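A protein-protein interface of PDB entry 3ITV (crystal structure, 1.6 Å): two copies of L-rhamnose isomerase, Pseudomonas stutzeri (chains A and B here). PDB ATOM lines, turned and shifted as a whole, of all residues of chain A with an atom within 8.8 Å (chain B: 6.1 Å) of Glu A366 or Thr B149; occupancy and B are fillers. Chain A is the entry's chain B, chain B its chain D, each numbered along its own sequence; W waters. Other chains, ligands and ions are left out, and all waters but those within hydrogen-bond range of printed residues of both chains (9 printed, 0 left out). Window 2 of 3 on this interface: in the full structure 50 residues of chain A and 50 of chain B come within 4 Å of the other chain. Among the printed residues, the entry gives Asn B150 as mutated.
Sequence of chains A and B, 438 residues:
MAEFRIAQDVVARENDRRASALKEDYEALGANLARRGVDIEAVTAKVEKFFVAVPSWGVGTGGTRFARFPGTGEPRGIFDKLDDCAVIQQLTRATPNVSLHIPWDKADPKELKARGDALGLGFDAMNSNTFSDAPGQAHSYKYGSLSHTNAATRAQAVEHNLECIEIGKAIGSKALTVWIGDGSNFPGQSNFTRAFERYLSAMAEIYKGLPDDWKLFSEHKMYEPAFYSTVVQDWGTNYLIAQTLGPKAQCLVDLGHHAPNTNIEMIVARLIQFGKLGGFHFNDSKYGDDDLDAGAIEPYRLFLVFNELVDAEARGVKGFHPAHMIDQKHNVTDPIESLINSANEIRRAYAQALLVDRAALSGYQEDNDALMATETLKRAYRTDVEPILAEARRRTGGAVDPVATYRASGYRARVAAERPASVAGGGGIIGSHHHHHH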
ATOM      1  N   ALA A 359      -7.715  19.517  21.206  1.00  0.00           N
ATOM      2  CA  ALA A 359      -6.534  18.661  21.112  1.00  0.00           C
ATOM      3  C   ALA A 359      -6.505  17.669  22.271  1.00  0.00           C
ATOM      4  O   ALA A 359      -6.281  16.473  22.074  1.00  0.00           O
ATOM      5  CB  ALA A 359      -5.265  19.511  21.116  1.00  0.00           C
ATOM      6  N   ALA A 360      -6.730  18.171  23.481  1.00  0.00           N
ATOM      7  CA  ALA A 360      -6.737  17.321  24.665  1.00  0.00           C
ATOM      8  C   ALA A 360      -7.865  16.301  24.570  1.00  0.00           C
ATOM      9  O   ALA A 360      -7.674  15.120  24.866  1.00  0.00           O
ATOM     10  CB  ALA A 360      -6.904  18.170  25.919  1.00  0.00           C
ATOM     11  N   LEU A 361      -9.042  16.759  24.157  1.00  0.00           N
ATOM     12  CA  LEU A 361     -10.190  15.868  24.033  1.00  0.00           C
ATOM     13  C   LEU A 361      -9.897  14.732  23.054  1.00  0.00           C
ATOM     14  O   LEU A 361     -10.179  13.570  23.340  1.00  0.00           O
ATOM     15  CB  LEU A 361     -11.424  16.646  23.567  1.00  0.00           C
ATOM     16  CG  LEU A 361     -12.708  15.821  23.433  1.00  0.00           C
ATOM     17  CD1 LEU A 361     -13.080  15.179  24.769  1.00  0.00           C
ATOM     18  CD2 LEU A 361     -13.823  16.723  22.953  1.00  0.00           C
ATOM     19  N   SER A 362      -9.332  15.073  21.899  1.00  0.00           N
ATOM     20  CA  SER A 362      -9.006  14.068  20.894  1.00  0.00           C
ATOM     21  C   SER A 362      -8.049  13.033  21.476  1.00  0.00           C
ATOM     22  O   SER A 362      -8.176  11.835  21.214  1.00  0.00           O
ATOM     23  CB  SER A 362      -8.372  14.733  19.670  1.00  0.00           C
ATOM     24  OG  SER A 362      -7.902  13.759  18.753  1.00  0.00           O
ATOM     25  N   GLY A 363      -7.092  13.505  22.269  1.00  0.00           N
ATOM     26  CA  GLY A 363      -6.132  12.608  22.885  1.00  0.00           C
ATOM     27  C   GLY A 363      -6.790  11.630  23.837  1.00  0.00           C
ATOM     28  O   GLY A 363      -6.488  10.436  23.821  1.00  0.00           O
ATOM     29  N   TYR A 364      -7.696  12.133  24.671  1.00  0.00           N
ATOM     30  CA  TYR A 364      -8.385  11.279  25.628  1.00  0.00           C
ATOM     31  C   TYR A 364      -9.347  10.318  24.936  1.00  0.00           C
ATOM     32  O   TYR A 364      -9.610   9.226  25.438  1.00  0.00           O
ATOM     33  CB  TYR A 364      -9.129  12.132  26.660  1.00  0.00           C
ATOM     34  CG  TYR A 364      -8.205  12.921  27.564  1.00  0.00           C
ATOM     35  CD1 TYR A 364      -7.152  12.297  28.234  1.00  0.00           C
ATOM     36  CD2 TYR A 364      -8.390  14.289  27.761  1.00  0.00           C
ATOM     37  CE1 TYR A 364      -6.305  13.017  29.078  1.00  0.00           C
ATOM     38  CE2 TYR A 364      -7.553  15.017  28.603  1.00  0.00           C
ATOM     39  CZ  TYR A 364      -6.514  14.376  29.256  1.00  0.00           C
ATOM     40  OH  TYR A 364      -5.686  15.098  30.087  1.00  0.00           O
ATOM     41  N   GLN A 365      -9.872  10.724  23.786  1.00  0.00           N
ATOM     42  CA  GLN A 365     -10.778   9.859  23.043  1.00  0.00           C
ATOM     43  C   GLN A 365      -9.988   8.714  22.424  1.00  0.00           C
ATOM     44  O   GLN A 365     -10.395   7.556  22.498  1.00  0.00           O
ATOM     45  CB  GLN A 365     -11.508  10.655  21.960  1.00  0.00           C
ATOM     46  CG  GLN A 365     -12.394  11.747  22.538  1.00  0.00           C
ATOM     47  CD  GLN A 365     -13.111  12.556  21.479  1.00  0.00           C
ATOM     48  OE1 GLN A 365     -12.554  12.814  20.415  1.00  0.00           O
ATOM     49  NE2 GLN A 365     -14.335  12.980  21.772  1.00  0.00           N
ATOM     50  N   GLU A 366      -8.846   9.035  21.826  1.00  0.00           N
ATOM     51  CA  GLU A 366      -8.020   8.003  21.211  1.00  0.00           C
ATOM     52  C   GLU A 366      -7.470   7.014  22.236  1.00  0.00           C
ATOM     53  O   GLU A 366      -7.340   5.824  21.947  1.00  0.00           O
ATOM     54  CB  GLU A 366      -6.868   8.640  20.429  1.00  0.00           C
ATOM     55  CG  GLU A 366      -7.311   9.317  19.143  1.00  0.00           C
ATOM     56  CD  GLU A 366      -8.103   8.383  18.242  1.00  0.00           C
ATOM     57  OE1 GLU A 366      -7.604   7.277  17.949  1.00  0.00           O
ATOM     58  OE2 GLU A 366      -9.221   8.754  17.824  1.00  0.00           O
ATOM     59  N   ASP A 367      -7.161   7.501  23.434  1.00  0.00           N
ATOM     60  CA  ASP A 367      -6.621   6.637  24.481  1.00  0.00           C
ATOM     61  C   ASP A 367      -7.695   5.997  25.352  1.00  0.00           C
ATOM     62  O   ASP A 367      -7.388   5.305  26.323  1.00  0.00           O
ATOM     63  CB  ASP A 367      -5.649   7.418  25.366  1.00  0.00           C
ATOM     64  CG  ASP A 367      -4.457   7.943  24.592  1.00  0.00           C
ATOM     65  OD1 ASP A 367      -3.903   7.184  23.769  1.00  0.00           O
ATOM     66  OD2 ASP A 367      -4.071   9.109  24.811  1.00  0.00           O
ATOM     67  N   ASN A 368      -8.956   6.229  24.999  1.00  0.00           N
ATOM     68  CA  ASN A 368     -10.077   5.671  25.746  1.00  0.00           C
ATOM     69  C   ASN A 368     -10.049   6.034  27.227  1.00  0.00           C
ATOM     70  O   ASN A 368     -10.368   5.215  28.090  1.00  0.00           O
ATOM     71  CB  ASN A 368     -10.125   4.146  25.576  1.00  0.00           C
ATOM     72  CG  ASN A 368     -10.425   3.734  24.146  1.00  0.00           C
ATOM     73  OD1 ASN A 368      -9.607   3.066  23.504  1.00  0.00           O
ATOM     74  ND2 ASN A 368     -11.585   4.131  23.640  1.00  0.00           N
ATOM     75  N   ASP A 369      -9.655   7.273  27.507  1.00  0.00           N
ATOM     76  CA  ASP A 369      -9.613   7.795  28.869  1.00  0.00           C
ATOM     77  C   ASP A 369     -10.948   8.524  29.010  1.00  0.00           C
ATOM     78  O   ASP A 369     -11.019   9.748  28.901  1.00  0.00           O
ATOM     79  CB  ASP A 369      -8.448   8.782  29.011  1.00  0.00           C
ATOM     80  CG  ASP A 369      -8.223   9.232  30.443  1.00  0.00           C
ATOM     81  OD1 ASP A 369      -9.129   9.054  31.285  1.00  0.00           O
ATOM     82  OD2 ASP A 369      -7.134   9.779  30.719  1.00  0.00           O
ATOM     83  N   ALA A 370     -12.006   7.754  29.239  1.00  0.00           N
ATOM     84  CA  ALA A 370     -13.358   8.293  29.351  1.00  0.00           C
ATOM     85  C   ALA A 370     -13.544   9.365  30.419  1.00  0.00           C
ATOM     86  O   ALA A 370     -14.255  10.353  30.199  1.00  0.00           O
ATOM     87  CB  ALA A 370     -14.345   7.153  29.585  1.00  0.00           C
ATOM     88  N   ALA A 373     -11.862  12.572  29.297  1.00  0.00           N
ATOM     89  CA  ALA A 373     -12.532  13.098  28.113  1.00  0.00           C
ATOM     90  C   ALA A 373     -13.757  13.879  28.577  1.00  0.00           C
ATOM     91  O   ALA A 373     -13.996  15.006  28.140  1.00  0.00           O
ATOM     92  CB  ALA A 373     -12.953  11.962  27.179  1.00  0.00           C
ATOM     93  N   TYR B 143     -13.594  -1.176  25.445  1.00  0.00           N
ATOM     94  CA  TYR B 143     -13.888   0.130  24.872  1.00  0.00           C
ATOM     95  C   TYR B 143     -14.412   0.067  23.442  1.00  0.00           C
ATOM     96  O   TYR B 143     -14.355   1.054  22.708  1.00  0.00           O
ATOM     97  CB  TYR B 143     -12.640   1.011  24.930  1.00  0.00           C
ATOM     98  CG  TYR B 143     -12.123   1.220  26.332  1.00  0.00           C
ATOM     99  CD1 TYR B 143     -12.867   1.935  27.270  1.00  0.00           C
ATOM    100  CD2 TYR B 143     -10.894   0.692  26.728  1.00  0.00           C
ATOM    101  CE1 TYR B 143     -12.403   2.119  28.570  1.00  0.00           C
ATOM    102  CE2 TYR B 143     -10.421   0.869  28.024  1.00  0.00           C
ATOM    103  CZ  TYR B 143     -11.179   1.584  28.938  1.00  0.00           C
ATOM    104  OH  TYR B 143     -10.712   1.760  30.221  1.00  0.00           O
ATOM    105  N   SER B 147     -15.759  -0.587  16.182  1.00  0.00           N
ATOM    106  CA  SER B 147     -15.540   0.859  16.164  1.00  0.00           C
ATOM    107  C   SER B 147     -14.476   1.312  17.167  1.00  0.00           C
ATOM    108  O   SER B 147     -14.323   2.505  17.417  1.00  0.00           O
ATOM    109  CB  SER B 147     -16.852   1.614  16.442  1.00  0.00           C
ATOM    110  OG  SER B 147     -17.280   1.460  17.788  1.00  0.00           O
ATOM    111  N   HIS B 148     -13.744   0.357  17.730  1.00  0.00           N
ATOM    112  CA  HIS B 148     -12.688   0.652  18.701  1.00  0.00           C
ATOM    113  C   HIS B 148     -11.652   1.582  18.064  1.00  0.00           C
ATOM    114  O   HIS B 148     -11.421   1.525  16.858  1.00  0.00           O
ATOM    115  CB  HIS B 148     -12.029  -0.661  19.136  1.00  0.00           C
ATOM    116  CG  HIS B 148     -11.228  -0.559  20.398  1.00  0.00           C
ATOM    117  ND1 HIS B 148     -10.010   0.083  20.462  1.00  0.00           N
ATOM    118  CD2 HIS B 148     -11.471  -1.032  21.642  1.00  0.00           C
ATOM    119  CE1 HIS B 148      -9.534  -0.004  21.691  1.00  0.00           C
ATOM    120  NE2 HIS B 148     -10.402  -0.676  22.428  1.00  0.00           N
ATOM    121  N   THR B 149     -11.036   2.444  18.867  1.00  0.00           N
ATOM    122  CA  THR B 149     -10.034   3.364  18.345  1.00  0.00           C
ATOM    123  C   THR B 149      -8.770   2.637  17.879  1.00  0.00           C
ATOM    124  O   THR B 149      -8.046   3.140  17.024  1.00  0.00           O
ATOM    125  CB  THR B 149      -9.628   4.409  19.398  1.00  0.00           C
ATOM    126  OG1 THR B 149      -9.136   3.741  20.567  1.00  0.00           O
ATOM    127  CG2 THR B 149     -10.820   5.278  19.775  1.00  0.00           C
ATOM    128  N   ASN B 150      -8.512   1.461  18.443  1.00  0.00           N
ATOM    129  CA  ASN B 150      -7.328   0.681  18.088  1.00  0.00           C
ATOM    130  C   ASN B 150      -7.549  -0.179  16.841  1.00  0.00           C
ATOM    131  O   ASN B 150      -8.423  -1.041  16.821  1.00  0.00           O
ATOM    132  CB  ASN B 150      -6.928  -0.209  19.265  1.00  0.00           C
ATOM    133  CG  ASN B 150      -5.644  -0.964  19.012  1.00  0.00           C
ATOM    134  OD1 ASN B 150      -4.610  -0.351  18.741  1.00  0.00           O
ATOM    135  ND2 ASN B 150      -5.697  -2.286  19.107  1.00  0.00           N
ATOM    136  N   ALA B 151      -6.742   0.049  15.813  1.00  0.00           N
ATOM    137  CA  ALA B 151      -6.861  -0.689  14.560  1.00  0.00           C
ATOM    138  C   ALA B 151      -6.777  -2.203  14.730  1.00  0.00           C
ATOM    139  O   ALA B 151      -7.534  -2.948  14.103  1.00  0.00           O
ATOM    140  CB  ALA B 151      -5.788  -0.214  13.578  1.00  0.00           C
ATOM    141  N   ARG B 154     -10.054  -3.573  16.015  1.00  0.00           N
ATOM    142  CA  ARG B 154     -11.083  -3.611  14.980  1.00  0.00           C
ATOM    143  C   ARG B 154     -10.833  -4.802  14.055  1.00  0.00           C
ATOM    144  O   ARG B 154     -11.763  -5.508  13.674  1.00  0.00           O
ATOM    145  CB  ARG B 154     -11.085  -2.316  14.154  1.00  0.00           C
ATOM    146  CG  ARG B 154     -11.419  -1.063  14.955  1.00  0.00           C
ATOM    147  CD  ARG B 154     -11.846   0.088  14.055  1.00  0.00           C
ATOM    148  NE  ARG B 154     -10.797   0.514  13.127  1.00  0.00           N
ATOM    149  CZ  ARG B 154      -9.758   1.277  13.460  1.00  0.00           C
ATOM    150  NH1 ARG B 154      -9.613   1.710  14.705  1.00  0.00           N
ATOM    151  NH2 ARG B 154      -8.861   1.613  12.541  1.00  0.00           N
ATOM    152  N   GLN B 189     -16.445  11.026  25.781  1.00  0.00           N
ATOM    153  CA  GLN B 189     -15.674   9.786  25.716  1.00  0.00           C
ATOM    154  C   GLN B 189     -15.420   9.370  24.273  1.00  0.00           C
ATOM    155  O   GLN B 189     -14.319   8.935  23.925  1.00  0.00           O
ATOM    156  CB  GLN B 189     -16.404   8.659  26.451  1.00  0.00           C
ATOM    157  CG  GLN B 189     -15.728   7.295  26.305  1.00  0.00           C
ATOM    158  CD  GLN B 189     -16.481   6.179  27.001  1.00  0.00           C
ATOM    159  OE1 GLN B 189     -16.125   5.007  26.857  1.00  0.00           O
ATOM    160  NE2 GLN B 189     -17.512   6.529  27.757  1.00  0.00           N
ATOM    161  N   ARG B 194     -16.462  10.044  14.290  1.00  0.00           N
ATOM    162  CA  ARG B 194     -15.294   9.204  14.057  1.00  0.00           C
ATOM    163  C   ARG B 194     -15.562   7.746  14.428  1.00  0.00           C
ATOM    164  O   ARG B 194     -15.119   6.835  13.728  1.00  0.00           O
ATOM    165  CB  ARG B 194     -14.079   9.739  14.825  1.00  0.00           C
ATOM    166  CG  ARG B 194     -13.580  11.085  14.310  1.00  0.00           C
ATOM    167  CD  ARG B 194     -12.093  11.264  14.580  1.00  0.00           C
ATOM    168  NE  ARG B 194     -11.577  12.513  14.022  1.00  0.00           N
ATOM    169  CZ  ARG B 194     -11.707  13.705  14.597  1.00  0.00           C
ATOM    170  NH1 ARG B 194     -12.337  13.821  15.758  1.00  0.00           N
ATOM    171  NH2 ARG B 194     -11.208  14.785  14.009  1.00  0.00           N
ATOM    172  N   ARG B 198     -15.393   4.576  11.840  1.00  0.00           N
ATOM    173  CA  ARG B 198     -14.607   3.369  12.085  1.00  0.00           C
ATOM    174  C   ARG B 198     -15.489   2.133  11.936  1.00  0.00           C
ATOM    175  O   ARG B 198     -15.083   1.126  11.350  1.00  0.00           O
ATOM    176  CB  ARG B 198     -13.979   3.407  13.482  1.00  0.00           C
ATOM    177  CG  ARG B 198     -12.886   4.465  13.632  1.00  0.00           C
ATOM    178  CD  ARG B 198     -12.106   4.299  14.931  1.00  0.00           C
ATOM    179  NE  ARG B 198     -12.894   4.583  16.129  1.00  0.00           N
ATOM    180  CZ  ARG B 198     -13.030   5.792  16.673  1.00  0.00           C
ATOM    181  NH1 ARG B 198     -12.435   6.842  16.127  1.00  0.00           N
ATOM    182  NH2 ARG B 198     -13.753   5.945  17.777  1.00  0.00           N
HETATM  183  O   HOH W   1     -12.963   7.476  22.064  1.00  0.00           O
HETATM  184  O   HOH W   2      -8.815   5.637  15.929  1.00  0.00           O
HETATM  185  O   HOH W   3     -14.275   4.344  24.656  1.00  0.00           O
HETATM  186  O   HOH W   4     -12.475   2.730  21.489  1.00  0.00           O
HETATM  187  O   HOH W   5     -11.533   5.034  30.633  1.00  0.00           O
HETATM  188  O   HOH W   6     -12.453   8.187  25.956  1.00  0.00           O
HETATM  189  O   HOH W   7      -6.048   3.406  20.282  1.00  0.00           O
HETATM  190  O   HOH W   8     -11.590  11.959  18.017  1.00  0.00           O
HETATM  191  O   HOH W   9     -11.784   9.277  17.897  1.00  0.00           O
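Among the printed residues, merely in contact across the chains: Ala A370 with Gln B189 (3.5 Å), Asn A368 with Tyr B143 (3.5 Å), Asn A368 with His B148 (3.6 Å), Gln A365 with Thr B149 (3.6 Å), Gln A365 with Gln B189 (3.7 Å) and Ala A373 with Gln B189 (3.8 Å).
The backbone NH (N) of Asn B150 is in hydrogen-bond range of a ring nitrogen (ND1) of His B148 (2.9 Å). The backbone carbonyl oxygen (O) of His B148 sits at hydrogen-bond distance from the guanidinium group (NH1) of Arg B154. The backbone carbonyl oxygen of His B148 lies close to the guanidinium group of Arg B198, 3.5 Å away. NH1 of Arg B154 is in hydrogen-bond range of O of Thr B149 (3.1 Å).
The backbone carbonyl oxygen (O) of Glu A366 is in hydrogen-bond range of the side-chain hydroxyl (OG1) of Thr B149. OD1 of Asn A368 lies within hydrogen-bond range of OG1 of Thr B149.
Ser A362 touches none of the printed residues of chain B. Of the printed residues of chain B, Gln A365 touches Thr B149 and Gln B189. Of chain B, only Thr B149 comes within 4 Å of Glu A366. Of the printed residues of chain B, Ala A373 touches Gln B189 (3.8 Å). Printed residues of chain A within 4 Å of His B148: Asn A368 (3.6 Å). Of the printed residues of chain A, Thr B149 touches Gln A365, Glu A366 and Asn A368. The nearest residue of chain B that does not touch Glu A366 is Arg B198 (4.1 Å).
Water W9 lies within hydrogen-bond range of the side-chain carboxylate (OE2) of Glu A366 (2.6 Å) and the guanidinium group (NH1) of Arg B198 (3.1 Å). Water W4 lies within hydrogen-bond range of ND2 of Asn A368, O of Tyr B143 and N of Thr B149. Water W5 lies within hydrogen-bond range of O of Asn A368 (2.8 Å), N of Ala A370 (3.1 Å) and OH of Tyr B143 (3.4 Å). Water W2 bridges O of Thr B149 and OE1 of Glu A366. Water W3 bridges the side-chain amide nitrogen (ND2) of Asn A368 (2.9 Å) and the side-chain amide oxygen (OE1) of Gln B189 (3.0 Å). Water W7 bridges OG1 of Thr B149 (3.1 Å) and O of Glu A366 (3.2 Å).
Of the 10 printed residues of chain B, 4 touch a printed residue of chain A. Hydrophobic or aromatic side chains of chain B within 4 Å of the printed part of chain A: Tyr B143 and His B148. Of the 13 printed residues of chain A, 5 touch a printed residue of chain B. Among the printed residues, no Asp or Glu carboxylate lies within 4 Å of a Lys or Arg side-chain nitrogen of the other chain.
No position is printed for both chains.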
